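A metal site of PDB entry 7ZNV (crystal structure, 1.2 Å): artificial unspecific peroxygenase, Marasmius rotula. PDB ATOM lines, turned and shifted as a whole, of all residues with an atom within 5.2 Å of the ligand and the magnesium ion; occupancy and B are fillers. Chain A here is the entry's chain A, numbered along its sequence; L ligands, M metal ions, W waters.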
ATOM      1  N   PRO A  23      22.048   4.731 -18.812  1.00  0.00           N
ATOM      2  CA  PRO A  23      22.296   3.627 -17.905  1.00  0.00           C
ATOM      3  C   PRO A  23      21.084   2.717 -17.677  1.00  0.00           C
ATOM      4  O   PRO A  23      21.118   1.862 -16.820  1.00  0.00           O
ATOM      5  CB  PRO A  23      22.735   4.311 -16.610  1.00  0.00           C
ATOM      6  CG  PRO A  23      22.935   5.776 -16.947  1.00  0.00           C
ATOM      7  CD  PRO A  23      21.972   6.011 -18.094  1.00  0.00           C
ATOM      8  N   CYS A  24      20.002   2.973 -18.420  1.00  0.00           N
ATOM      9  CA  CYS A  24      18.690   2.348 -18.188  1.00  0.00           C
ATOM     10  C   CYS A  24      18.387   1.316 -19.237  1.00  0.00           C
ATOM     11  O   CYS A  24      18.243   1.645 -20.424  1.00  0.00           O
ATOM     12  CB  CYS A  24      17.599   3.395 -18.241  1.00  0.00           C
ATOM     13  SG  CYS A  24      15.946   2.678 -18.030  1.00  0.00           S
ATOM     14  N   PRO A  25      18.326   0.024 -18.903  1.00  0.00           N
ATOM     15  CA  PRO A  25      17.953  -0.986 -19.897  1.00  0.00           C
ATOM     16  C   PRO A  25      16.538  -0.754 -20.415  1.00  0.00           C
ATOM     17  O   PRO A  25      16.251  -1.140 -21.560  1.00  0.00           O
ATOM     18  CB  PRO A  25      18.097  -2.301 -19.139  1.00  0.00           C
ATOM     19  CG  PRO A  25      17.811  -1.932 -17.709  1.00  0.00           C
ATOM     20  CD  PRO A  25      18.457  -0.554 -17.547  1.00  0.00           C
ATOM     21  N   GLY A  26      15.657  -0.172 -19.602  1.00  0.00           N
ATOM     22  CA  GLY A  26      14.284   0.070 -20.038  1.00  0.00           C
ATOM     23  C   GLY A  26      14.249   1.016 -21.210  1.00  0.00           C
ATOM     24  O   GLY A  26      13.665   0.722 -22.282  1.00  0.00           O
ATOM     25  N   LEU A  27      14.811   2.190 -21.061  1.00  0.00           N
ATOM     26  CA  LEU A  27      14.826   3.176 -22.140  1.00  0.00           C
ATOM     27  C   LEU A  27      15.682   2.715 -23.287  1.00  0.00           C
ATOM     28  O   LEU A  27      15.354   2.974 -24.449  1.00  0.00           O
ATOM     29  CB  LEU A  27      15.263   4.542 -21.628  1.00  0.00           C
ATOM     30  CG  LEU A  27      14.450   5.154 -20.490  1.00  0.00           C
ATOM     31  CD1 LEU A  27      14.982   6.562 -20.242  1.00  0.00           C
ATOM     32  CD2 LEU A  27      12.964   5.168 -20.831  1.00  0.00           C
ATOM     33  N   LEU A  30      13.821   0.347 -25.507  1.00  0.00           N
ATOM     34  CA  LEU A  30      12.829   1.090 -26.267  1.00  0.00           C
ATOM     35  C   LEU A  30      13.520   1.770 -27.432  1.00  0.00           C
ATOM     36  O   LEU A  30      12.947   1.777 -28.568  1.00  0.00           O
ATOM     37  CB  LEU A  30      12.077   2.091 -25.409  1.00  0.00           C
ATOM     38  CG  LEU A  30      11.194   1.480 -24.361  1.00  0.00           C
ATOM     39  CD1 LEU A  30      10.642   2.550 -23.403  1.00  0.00           C
ATOM     40  CD2 LEU A  30      10.035   0.655 -24.921  1.00  0.00           C
ATOM     41  N   ILE A  48       8.645   9.765 -23.922  1.00  0.00           N
ATOM     42  CA  ILE A  48       8.916   8.710 -22.930  1.00  0.00           C
ATOM     43  C   ILE A  48       7.599   8.029 -22.572  1.00  0.00           C
ATOM     44  O   ILE A  48       7.535   6.795 -22.491  1.00  0.00           O
ATOM     45  CB  ILE A  48       9.531   9.340 -21.662  1.00  0.00           C
ATOM     46  CG1 ILE A  48      10.950   9.826 -21.947  1.00  0.00           C
ATOM     47  CG2 ILE A  48       9.427   8.358 -20.501  1.00  0.00           C
ATOM     48  CD1 ILE A  48      11.970   8.740 -22.066  1.00  0.00           C
ATOM     49  N   GLY A  52       6.990   4.050 -23.328  1.00  0.00           N
ATOM     50  CA  GLY A  52       6.795   3.091 -22.246  1.00  0.00           C
ATOM     51  C   GLY A  52       5.469   2.377 -22.370  1.00  0.00           C
ATOM     52  O   GLY A  52       5.375   1.188 -22.062  1.00  0.00           O
ATOM     53  N   TYR A  56       5.915  -1.576 -23.351  1.00  0.00           N
ATOM     54  CA  TYR A  56       5.802  -2.350 -22.104  1.00  0.00           C
ATOM     55  C   TYR A  56       4.455  -2.363 -21.447  1.00  0.00           C
ATOM     56  O   TYR A  56       4.267  -3.052 -20.485  1.00  0.00           O
ATOM     57  CB  TYR A  56       6.823  -1.816 -21.076  1.00  0.00           C
ATOM     58  CG  TYR A  56       8.274  -1.766 -21.477  1.00  0.00           C
ATOM     59  CD1 TYR A  56       8.932  -2.851 -22.066  1.00  0.00           C
ATOM     60  CD2 TYR A  56       9.065  -0.654 -21.171  1.00  0.00           C
ATOM     61  CE1 TYR A  56      10.276  -2.806 -22.356  1.00  0.00           C
ATOM     62  CE2 TYR A  56      10.416  -0.596 -21.463  1.00  0.00           C
ATOM     63  CZ  TYR A  56      10.997  -1.667 -22.072  1.00  0.00           C
ATOM     64  OH  TYR A  56      12.348  -1.652 -22.413  1.00  0.00           O
ATOM     65  N   VAL A  58       3.510   0.183 -19.775  1.00  0.00           N
ATOM     66  CA  VAL A  58       3.709   1.002 -18.545  1.00  0.00           C
ATOM     67  C   VAL A  58       2.934   2.299 -18.722  1.00  0.00           C
ATOM     68  O   VAL A  58       2.989   2.941 -19.742  1.00  0.00           O
ATOM     69  CB  VAL A  58       5.210   1.190 -18.282  1.00  0.00           C
ATOM     70  CG1 VAL A  58       5.419   2.179 -17.132  1.00  0.00           C
ATOM     71  CG2 VAL A  58       5.891  -0.121 -17.991  1.00  0.00           C
ATOM     72  N   LEU A  63       6.183   7.179 -15.320  1.00  0.00           N
ATOM     73  CA  LEU A  63       7.037   7.645 -16.376  1.00  0.00           C
ATOM     74  C   LEU A  63       7.156   9.167 -16.365  1.00  0.00           C
ATOM     75  O   LEU A  63       8.196   9.671 -16.684  1.00  0.00           O
ATOM     76  CB  LEU A  63       6.482   7.165 -17.693  1.00  0.00           C
ATOM     77  CG  LEU A  63       6.450   5.659 -17.892  1.00  0.00           C
ATOM     78  CD1 LEU A  63       5.792   5.319 -19.257  1.00  0.00           C
ATOM     79  CD2 LEU A  63       7.852   5.068 -17.811  1.00  0.00           C
ATOM     80  N   ALA A  66       9.639  10.381 -13.535  1.00  0.00           N
ATOM     81  CA  ALA A  66      11.005  10.028 -13.921  1.00  0.00           C
ATOM     82  C   ALA A  66      11.514  10.913 -15.047  1.00  0.00           C
ATOM     83  O   ALA A  66      12.638  11.343 -15.029  1.00  0.00           O
ATOM     84  CB  ALA A  66      11.098   8.568 -14.276  1.00  0.00           C
ATOM     85  N   ALA A  67      10.653  11.134 -16.053  1.00  0.00           N
ATOM     86  CA  ALA A  67      11.059  11.944 -17.179  1.00  0.00           C
ATOM     87  C   ALA A  67      11.278  13.420 -16.800  1.00  0.00           C
ATOM     88  O   ALA A  67      12.189  14.044 -17.300  1.00  0.00           O
ATOM     89  CB  ALA A  67      10.070  11.845 -18.315  1.00  0.00           C
ATOM     90  N   GLY A  70      14.496  13.434 -15.198  1.00  0.00           N
ATOM     91  CA  GLY A  70      15.494  13.256 -16.225  1.00  0.00           C
ATOM     92  C   GLY A  70      15.803  14.544 -16.961  1.00  0.00           C
ATOM     93  O   GLY A  70      16.954  14.743 -17.379  1.00  0.00           O
ATOM     94  N   PHE A  80      15.877  15.715 -23.315  1.00  0.00           N
ATOM     95  CA  PHE A  80      17.159  15.137 -22.952  1.00  0.00           C
ATOM     96  C   PHE A  80      17.579  14.150 -24.006  1.00  0.00           C
ATOM     97  O   PHE A  80      16.766  13.696 -24.827  1.00  0.00           O
ATOM     98  CB  PHE A  80      17.154  14.493 -21.558  1.00  0.00           C
ATOM     99  CG  PHE A  80      16.108  13.443 -21.288  1.00  0.00           C
ATOM    100  CD1 PHE A  80      16.206  12.189 -21.858  1.00  0.00           C
ATOM    101  CD2 PHE A  80      15.081  13.663 -20.396  1.00  0.00           C
ATOM    102  CE1 PHE A  80      15.237  11.223 -21.598  1.00  0.00           C
ATOM    103  CE2 PHE A  80      14.128  12.707 -20.119  1.00  0.00           C
ATOM    104  CZ  PHE A  80      14.194  11.490 -20.748  1.00  0.00           C
ATOM    105  N   LEU A  85      21.258  11.162 -19.127  1.00  0.00           N
ATOM    106  CA  LEU A  85      20.717  10.496 -17.936  1.00  0.00           C
ATOM    107  C   LEU A  85      21.793   9.807 -17.127  1.00  0.00           C
ATOM    108  O   LEU A  85      21.478   9.358 -16.003  1.00  0.00           O
ATOM    109  CB  LEU A  85      19.663   9.484 -18.357  1.00  0.00           C
ATOM    110  CG  LEU A  85      18.424  10.032 -19.071  1.00  0.00           C
ATOM    111  CD1 LEU A  85      17.525   8.888 -19.500  1.00  0.00           C
ATOM    112  CD2 LEU A  85      17.672  11.024 -18.215  1.00  0.00           C
ATOM    113  N   ILE A  91      19.235  10.763 -11.153  1.00  0.00           N
ATOM    114  CA  ILE A  91      18.611   9.430 -10.989  1.00  0.00           C
ATOM    115  C   ILE A  91      19.748   8.424 -10.797  1.00  0.00           C
ATOM    116  O   ILE A  91      19.659   7.597  -9.906  1.00  0.00           O
ATOM    117  CB  ILE A  91      17.752   9.048 -12.220  1.00  0.00           C
ATOM    118  CG1 ILE A  91      16.567  10.012 -12.387  1.00  0.00           C
ATOM    119  CG2 ILE A  91      17.299   7.605 -12.122  1.00  0.00           C
ATOM    120  CD1 ILE A  91      15.850   9.882 -13.709  1.00  0.00           C
ATOM    121  N   GLU A  92      20.756   8.485 -11.676  1.00  0.00           N
ATOM    122  CA  GLU A  92      21.875   7.514 -11.624  1.00  0.00           C
ATOM    123  C   GLU A  92      22.453   7.443 -10.204  1.00  0.00           C
ATOM    124  O   GLU A  92      22.710   8.476  -9.573  1.00  0.00           O
ATOM    125  CB  GLU A  92      22.890   7.822 -12.714  1.00  0.00           C
ATOM    126  CG  GLU A  92      23.845   6.677 -12.944  1.00  0.00           C
ATOM    127  CD  GLU A  92      24.904   6.474 -11.899  1.00  0.00           C
ATOM    128  OE1 GLU A  92      25.481   7.502 -11.459  1.00  0.00           O
ATOM    129  OE2 GLU A  92      25.180   5.334 -11.490  1.00  0.00           O
ATOM    130  N   HIS A  93      22.665   6.221  -9.779  1.00  0.00           N
ATOM    131  CA  HIS A  93      23.077   5.959  -8.380  1.00  0.00           C
ATOM    132  C   HIS A  93      24.046   4.780  -8.314  1.00  0.00           C
ATOM    133  O   HIS A  93      24.163   3.989  -9.258  1.00  0.00           O
ATOM    134  CB  HIS A  93      21.836   5.599  -7.552  1.00  0.00           C
ATOM    135  CG  HIS A  93      21.040   4.494  -8.172  1.00  0.00           C
ATOM    136  ND1 HIS A  93      21.447   3.166  -8.139  1.00  0.00           N
ATOM    137  CD2 HIS A  93      19.903   4.514  -8.901  1.00  0.00           C
ATOM    138  CE1 HIS A  93      20.584   2.427  -8.791  1.00  0.00           C
ATOM    139  NE2 HIS A  93      19.630   3.223  -9.265  1.00  0.00           N
ATOM    140  N   ASP A  94      24.743   4.721  -7.195  1.00  0.00           N
ATOM    141  CA  ASP A  94      25.604   3.579  -6.860  1.00  0.00           C
ATOM    142  C   ASP A  94      24.800   2.315  -6.644  1.00  0.00           C
ATOM    143  O   ASP A  94      23.561   2.373  -6.450  1.00  0.00           O
ATOM    144  CB  ASP A  94      26.385   3.957  -5.608  1.00  0.00           C
ATOM    145  CG  ASP A  94      27.245   5.167  -5.767  1.00  0.00           C
ATOM    146  OD1 ASP A  94      27.700   5.404  -6.870  1.00  0.00           O
ATOM    147  OD2 ASP A  94      27.451   5.872  -4.742  1.00  0.00           O
ATOM    148  N   SER A  96      24.159  -0.139  -8.703  1.00  0.00           N
ATOM    149  CA  SER A  96      23.374  -0.586  -9.864  1.00  0.00           C
ATOM    150  C   SER A  96      23.501  -2.075 -10.040  1.00  0.00           C
ATOM    151  O   SER A  96      24.457  -2.713  -9.590  1.00  0.00           O
ATOM    152  CB  SER A  96      23.785   0.143 -11.101  1.00  0.00           C
ATOM    153  OG  SER A  96      23.456   1.531 -11.016  1.00  0.00           O
ATOM    154  N   LEU A  97      22.545  -2.659 -10.764  1.00  0.00           N
ATOM    155  CA  LEU A  97      22.496  -4.084 -11.076  1.00  0.00           C
ATOM    156  C   LEU A  97      23.453  -4.492 -12.160  1.00  0.00           C
ATOM    157  O   LEU A  97      23.826  -5.679 -12.193  1.00  0.00           O
ATOM    158  CB  LEU A  97      21.082  -4.419 -11.582  1.00  0.00           C
ATOM    159  CG  LEU A  97      19.971  -4.136 -10.591  1.00  0.00           C
ATOM    160  CD1 LEU A  97      18.636  -4.190 -11.335  1.00  0.00           C
ATOM    161  CD2 LEU A  97      19.935  -5.078  -9.432  1.00  0.00           C
ATOM    162  N   SER A  98      23.856  -3.589 -13.021  1.00  0.00           N
ATOM    163  CA  SER A  98      24.567  -3.954 -14.236  1.00  0.00           C
ATOM    164  C   SER A  98      25.609  -2.944 -14.674  1.00  0.00           C
ATOM    165  O   SER A  98      26.202  -3.105 -15.746  1.00  0.00           O
ATOM    166  CB  SER A  98      23.630  -4.242 -15.365  1.00  0.00           C
ATOM    167  OG  SER A  98      22.957  -3.102 -15.835  1.00  0.00           O
ATOM    168  N   ARG A  99      25.783  -1.877 -13.904  1.00  0.00           N
ATOM    169  CA  ARG A  99      26.753  -0.809 -14.162  1.00  0.00           C
ATOM    170  C   ARG A  99      27.647  -0.686 -12.949  1.00  0.00           C
ATOM    171  O   ARG A  99      27.254  -0.985 -11.859  1.00  0.00           O
ATOM    172  CB  ARG A  99      26.054   0.526 -14.431  1.00  0.00           C
ATOM    173  CG  ARG A  99      25.640   0.821 -15.847  1.00  0.00           C
ATOM    174  CD  ARG A  99      24.622  -0.155 -16.432  1.00  0.00           C
ATOM    175  NE  ARG A  99      24.228   0.275 -17.729  1.00  0.00           N
ATOM    176  CZ  ARG A  99      23.442  -0.407 -18.570  1.00  0.00           C
ATOM    177  NH1 ARG A  99      23.000  -1.577 -18.222  1.00  0.00           N
ATOM    178  NH2 ARG A  99      23.175   0.091 -19.758  1.00  0.00           N
ATOM    179  N   GLU A 100      28.851  -0.148 -13.169  1.00  0.00           N
ATOM    180  CA  GLU A 100      29.769   0.202 -12.056  1.00  0.00           C
ATOM    181  C   GLU A 100      29.358   1.520 -11.442  1.00  0.00           C
ATOM    182  O   GLU A 100      28.710   2.353 -12.063  1.00  0.00           O
ATOM    183  CB  GLU A 100      31.190   0.290 -12.625  1.00  0.00           C
ATOM    184  CG  GLU A 100      31.692  -0.995 -13.240  1.00  0.00           C
ATOM    185  CD  GLU A 100      33.039  -0.912 -13.943  1.00  0.00           C
ATOM    186  OE1 GLU A 100      33.346   0.109 -14.571  1.00  0.00           O
ATOM    187  OE2 GLU A 100      33.743  -1.953 -13.921  1.00  0.00           O
ATOM    188  N   ASN A 107      29.690   4.251 -15.180  1.00  0.00           N
ATOM    189  CA  ASN A 107      28.307   4.245 -14.638  1.00  0.00           C
ATOM    190  C   ASN A 107      27.231   4.145 -15.716  1.00  0.00           C
ATOM    191  O   ASN A 107      26.047   4.256 -15.385  1.00  0.00           O
ATOM    192  CB  ASN A 107      28.021   5.430 -13.723  1.00  0.00           C
ATOM    193  CG  ASN A 107      27.793   6.710 -14.462  1.00  0.00           C
ATOM    194  OD1 ASN A 107      28.101   6.815 -15.673  1.00  0.00           O
ATOM    195  ND2 ASN A 107      27.227   7.720 -13.846  1.00  0.00           N
ATOM    196  N   GLU A 164      13.414   0.016  -9.672  1.00  0.00           N
ATOM    197  CA  GLU A 164      14.089  -0.530 -10.875  1.00  0.00           C
ATOM    198  C   GLU A 164      14.020  -2.058 -10.875  1.00  0.00           C
ATOM    199  O   GLU A 164      13.788  -2.638 -11.926  1.00  0.00           O
ATOM    200  CB  GLU A 164      15.523   0.006 -10.930  1.00  0.00           C
ATOM    201  CG  GLU A 164      15.500   1.451 -11.372  1.00  0.00           C
ATOM    202  CD  GLU A 164      16.726   2.313 -11.120  1.00  0.00           C
ATOM    203  OE1 GLU A 164      17.610   1.860 -10.396  1.00  0.00           O
ATOM    204  OE2 GLU A 164      16.760   3.446 -11.662  1.00  0.00           O
ATOM    205  N   SER A 165      14.179  -2.658  -9.709  1.00  0.00           N
ATOM    206  CA  SER A 165      14.103  -4.137  -9.645  1.00  0.00           C
ATOM    207  C   SER A 165      12.647  -4.567  -9.895  1.00  0.00           C
ATOM    208  O   SER A 165      12.426  -5.526 -10.619  1.00  0.00           O
ATOM    209  CB  SER A 165      14.692  -4.645  -8.343  1.00  0.00           C
ATOM    210  OG  SER A 165      16.114  -4.620  -8.417  1.00  0.00           O
ATOM    211  N   PHE A 167      10.672  -3.017 -11.804  1.00  0.00           N
ATOM    212  CA  PHE A 167      10.543  -2.809 -13.265  1.00  0.00           C
ATOM    213  C   PHE A 167      11.052  -4.030 -14.049  1.00  0.00           C
ATOM    214  O   PHE A 167      10.361  -4.451 -14.961  1.00  0.00           O
ATOM    215  CB  PHE A 167      11.246  -1.527 -13.698  1.00  0.00           C
ATOM    216  CG  PHE A 167      10.340  -0.339 -13.932  1.00  0.00           C
ATOM    217  CD1 PHE A 167       9.188  -0.450 -14.683  1.00  0.00           C
ATOM    218  CD2 PHE A 167      10.673   0.900 -13.415  1.00  0.00           C
ATOM    219  CE1 PHE A 167       8.371   0.655 -14.900  1.00  0.00           C
ATOM    220  CE2 PHE A 167       9.867   1.996 -13.637  1.00  0.00           C
ATOM    221  CZ  PHE A 167       8.720   1.874 -14.382  1.00  0.00           C
ATOM    222  N   TYR A 168      12.250  -4.536 -13.750  1.00  0.00           N
ATOM    223  CA  TYR A 168      12.750  -5.651 -14.615  1.00  0.00           C
ATOM    224  C   TYR A 168      11.849  -6.867 -14.395  1.00  0.00           C
ATOM    225  O   TYR A 168      11.560  -7.575 -15.352  1.00  0.00           O
ATOM    226  CB  TYR A 168      14.261  -5.944 -14.463  1.00  0.00           C
ATOM    227  CG  TYR A 168      14.737  -6.680 -13.231  1.00  0.00           C
ATOM    228  CD1 TYR A 168      14.493  -8.037 -13.058  1.00  0.00           C
ATOM    229  CD2 TYR A 168      15.498  -6.033 -12.275  1.00  0.00           C
ATOM    230  CE1 TYR A 168      14.954  -8.711 -11.943  1.00  0.00           C
ATOM    231  CE2 TYR A 168      15.962  -6.698 -11.148  1.00  0.00           C
ATOM    232  CZ  TYR A 168      15.691  -8.047 -10.984  1.00  0.00           C
ATOM    233  OH  TYR A 168      16.135  -8.721  -9.884  1.00  0.00           O
ATOM    234  N   VAL A 171       8.320  -5.868 -16.310  1.00  0.00           N
ATOM    235  CA  VAL A 171       8.265  -5.710 -17.776  1.00  0.00           C
ATOM    236  C   VAL A 171       8.748  -6.975 -18.457  1.00  0.00           C
ATOM    237  O   VAL A 171       8.188  -7.263 -19.549  1.00  0.00           O
ATOM    238  CB  VAL A 171       8.943  -4.457 -18.345  1.00  0.00           C
ATOM    239  CG1 VAL A 171       8.440  -3.271 -17.535  1.00  0.00           C
ATOM    240  CG2 VAL A 171      10.475  -4.461 -18.350  1.00  0.00           C
ATOM    241  N   PHE A 188      17.310  -8.920 -21.847  1.00  0.00           N
ATOM    242  CA  PHE A 188      16.967  -7.509 -21.622  1.00  0.00           C
ATOM    243  C   PHE A 188      18.220  -6.712 -21.226  1.00  0.00           C
ATOM    244  O   PHE A 188      18.499  -5.645 -21.792  1.00  0.00           O
ATOM    245  CB  PHE A 188      15.851  -7.449 -20.593  1.00  0.00           C
ATOM    246  CG  PHE A 188      15.379  -6.084 -20.166  1.00  0.00           C
ATOM    247  CD1 PHE A 188      14.728  -5.263 -21.050  1.00  0.00           C
ATOM    248  CD2 PHE A 188      15.496  -5.693 -18.839  1.00  0.00           C
ATOM    249  CE1 PHE A 188      14.240  -4.028 -20.590  1.00  0.00           C
ATOM    250  CE2 PHE A 188      15.016  -4.475 -18.396  1.00  0.00           C
ATOM    251  CZ  PHE A 188      14.380  -3.691 -19.291  1.00  0.00           C
ATOM    252  N   PHE A 189      18.932  -7.169 -20.221  1.00  0.00           N
ATOM    253  CA  PHE A 189      20.113  -6.439 -19.738  1.00  0.00           C
ATOM    254  C   PHE A 189      21.275  -6.541 -20.726  1.00  0.00           C
ATOM    255  O   PHE A 189      21.933  -5.545 -21.036  1.00  0.00           O
ATOM    256  CB  PHE A 189      20.534  -6.919 -18.372  1.00  0.00           C
ATOM    257  CG  PHE A 189      19.761  -6.343 -17.234  1.00  0.00           C
ATOM    258  CD1 PHE A 189      20.220  -5.181 -16.605  1.00  0.00           C
ATOM    259  CD2 PHE A 189      18.634  -6.933 -16.736  1.00  0.00           C
ATOM    260  CE1 PHE A 189      19.576  -4.672 -15.509  1.00  0.00           C
ATOM    261  CE2 PHE A 189      17.941  -6.377 -15.656  1.00  0.00           C
ATOM    262  CZ  PHE A 189      18.413  -5.228 -15.057  1.00  0.00           C
HETATM  263  C1  LIG L   1      18.004   2.308 -14.334  1.00  0.00           C
HETATM  264  C2  LIG L   1      14.188  -0.147 -15.976  1.00  0.00           C
HETATM  265  C3  LIG L   1      12.129   4.048 -17.333  1.00  0.00           C
HETATM  266  C4  LIG L   1      16.169   6.408 -16.115  1.00  0.00           C
HETATM  267  C5  LIG L   1      17.099   1.324 -14.585  1.00  0.00           C
HETATM  268  C6  LIG L   1      17.270  -0.017 -14.159  1.00  0.00           C
HETATM  269  C7  LIG L   1      16.196  -0.718 -14.607  1.00  0.00           C
HETATM  270  C8  LIG L   1      15.367   0.190 -15.315  1.00  0.00           C
HETATM  271  C9  LIG L   1      15.942  -2.194 -14.412  1.00  0.00           C
HETATM  272  C10 LIG L   1      18.426  -0.544 -13.341  1.00  0.00           C
HETATM  273  C11 LIG L   1      19.681  -0.787 -14.168  1.00  0.00           C
HETATM  274  C12 LIG L   1      20.815  -1.247 -13.288  1.00  0.00           C
HETATM  275  O1  LIG L   1      21.814  -1.750 -13.791  1.00  0.00           O
HETATM  276  O2  LIG L   1      20.737  -1.133 -12.047  1.00  0.00           O
HETATM  277  C13 LIG L   1      13.316   0.806 -16.519  1.00  0.00           C
HETATM  278  C14 LIG L   1      12.069   0.458 -17.109  1.00  0.00           C
HETATM  279  C15 LIG L   1      11.478   1.615 -17.502  1.00  0.00           C
HETATM  280  C16 LIG L   1      12.401   2.700 -17.125  1.00  0.00           C
HETATM  281  C17 LIG L   1      11.508  -0.936 -17.287  1.00  0.00           C
HETATM  282  C18 LIG L   1      10.162   1.760 -18.150  1.00  0.00           C
HETATM  283  C19 LIG L   1      10.021   2.504 -19.250  1.00  0.00           C
HETATM  284  C20 LIG L   1      13.014   5.076 -17.056  1.00  0.00           C
HETATM  285  C21 LIG L   1      12.752   6.444 -17.200  1.00  0.00           C
HETATM  286  C22 LIG L   1      13.902   7.113 -16.853  1.00  0.00           C
HETATM  287  C23 LIG L   1      14.876   6.133 -16.479  1.00  0.00           C
HETATM  288  C24 LIG L   1      11.422   7.033 -17.651  1.00  0.00           C
HETATM  289  C25 LIG L   1      14.123   8.580 -16.860  1.00  0.00           C
HETATM  290  C26 LIG L   1      13.682   9.318 -17.866  1.00  0.00           C
HETATM  291  C27 LIG L   1      17.000   5.434 -15.547  1.00  0.00           C
HETATM  292  C28 LIG L   1      18.341   5.768 -15.032  1.00  0.00           C
HETATM  293  C29 LIG L   1      18.839   4.630 -14.531  1.00  0.00           C
HETATM  294  C30 LIG L   1      17.809   3.614 -14.755  1.00  0.00           C
HETATM  295  C31 LIG L   1      19.024   7.125 -15.063  1.00  0.00           C
HETATM  296  C32 LIG L   1      20.189   4.427 -13.883  1.00  0.00           C
HETATM  297  C33 LIG L   1      20.054   4.207 -12.378  1.00  0.00           C
HETATM  298  C34 LIG L   1      21.264   3.435 -11.911  1.00  0.00           C
HETATM  299  O3  LIG L   1      22.261   4.025 -11.467  1.00  0.00           O
HETATM  300  O4  LIG L   1      21.245   2.196 -11.992  1.00  0.00           O
HETATM  301  N1  LIG L   1      15.912   1.435 -15.282  1.00  0.00           N
HETATM  302  N2  LIG L   1      13.460   2.133 -16.545  1.00  0.00           N
HETATM  303  N3  LIG L   1      14.286   4.911 -16.611  1.00  0.00           N
HETATM  304  N4  LIG L   1      16.718   4.130 -15.361  1.00  0.00           N
HETATM  305 FE1  LIG L   1      15.143   3.162 -15.884  1.00  0.00          FE
HETATM  306 MG    MG M   1      24.298   3.471 -11.311  1.00  0.00          MG
HETATM  307  O   HOH W   1      26.189   2.649 -10.975  1.00  0.00           O
HETATM  308  O   HOH W   2      19.214  -0.460  -9.877  1.00  0.00           O
HETATM  309  O   HOH W   3      22.608   1.569 -14.515  1.00  0.00           O
HETATM  310  O   HOH W   4      24.402   3.226 -13.358  1.00  0.00           O
HETATM  311  O   HOH W   5      14.445   3.544 -14.048  1.00  0.00           O
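The backbone NH of His 93 lies close to an oxygen (O3) of the ligand (2.8 Å).
A ring nitrogen (NE2) of His 93 sits close to an oxygen (O4) of the ligand.
SG of Cys 24 is bound to FE1 of the ligand.
N of Leu 97 sits at hydrogen-bond distance from O2 of the ligand (2.7 Å).
The backbone NH (N) of Ser 98 sits at hydrogen-bond distance from an oxygen (O1) of the ligand (2.9 Å).
The side-chain hydroxyl (OG) of Ser 98 is in hydrogen-bond range of an oxygen (O1) of the ligand, 2.7 Å away.
Residues that only touch the ligand: Pro 23, Pro 25, Gly 26, Leu 27, Ile 48, Tyr 56, Leu 63, Ala 66, Ala 67, Phe 80, Leu 85, Ile 91, Arg 99, Glu 164, Phe 167, Val 171 and Phe 189.
Of the 33 residues printed, 23 come within 4 Å of the ligand.
The nearest printed residue that does not touch the ligand is Tyr 168 (4.1 Å).
The magnesium ion is bound by water W4 (2.1 Å), OE2 of Glu 92 (2.1 Å), water W1 (2.1 Å), O3 of the ligand (2.1 Å), O of His 93 (2.1 Å) and OG of Ser 96 (2.1 Å).
The magnesium ion has six donor atoms within binding distance.
OE1 of Glu 92 is in hydrogen-bond range of ND2 of Asn 107.
OE1 of Glu 164 sits at hydrogen-bond distance from NE2 of His 93.
The side-chain sulfur (SG) of Cys 24 lies close to the backbone NH (N) of Leu 27 (3.3 Å).
N of Gly 26 lies close to SG of Cys 24.
OG of Ser 98 lies within hydrogen-bond range of NH1 of Arg 99, 2.8 Å away.
O of Gly 26 sits at hydrogen-bond distance from OH of Tyr 56 (2.7 Å).
The nearest printed residue that does not touch the magnesium ion is Asp 94 (4.3 Å).
Water W2 bridges O2 of the ligand (2.7 Å) and OE1 of Glu 164 (2.9 Å).
Water W3 bridges the backbone carbonyl oxygen (O) of Pro 23 (2.8 Å) and an oxygen (O4) of the ligand (2.9 Å).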
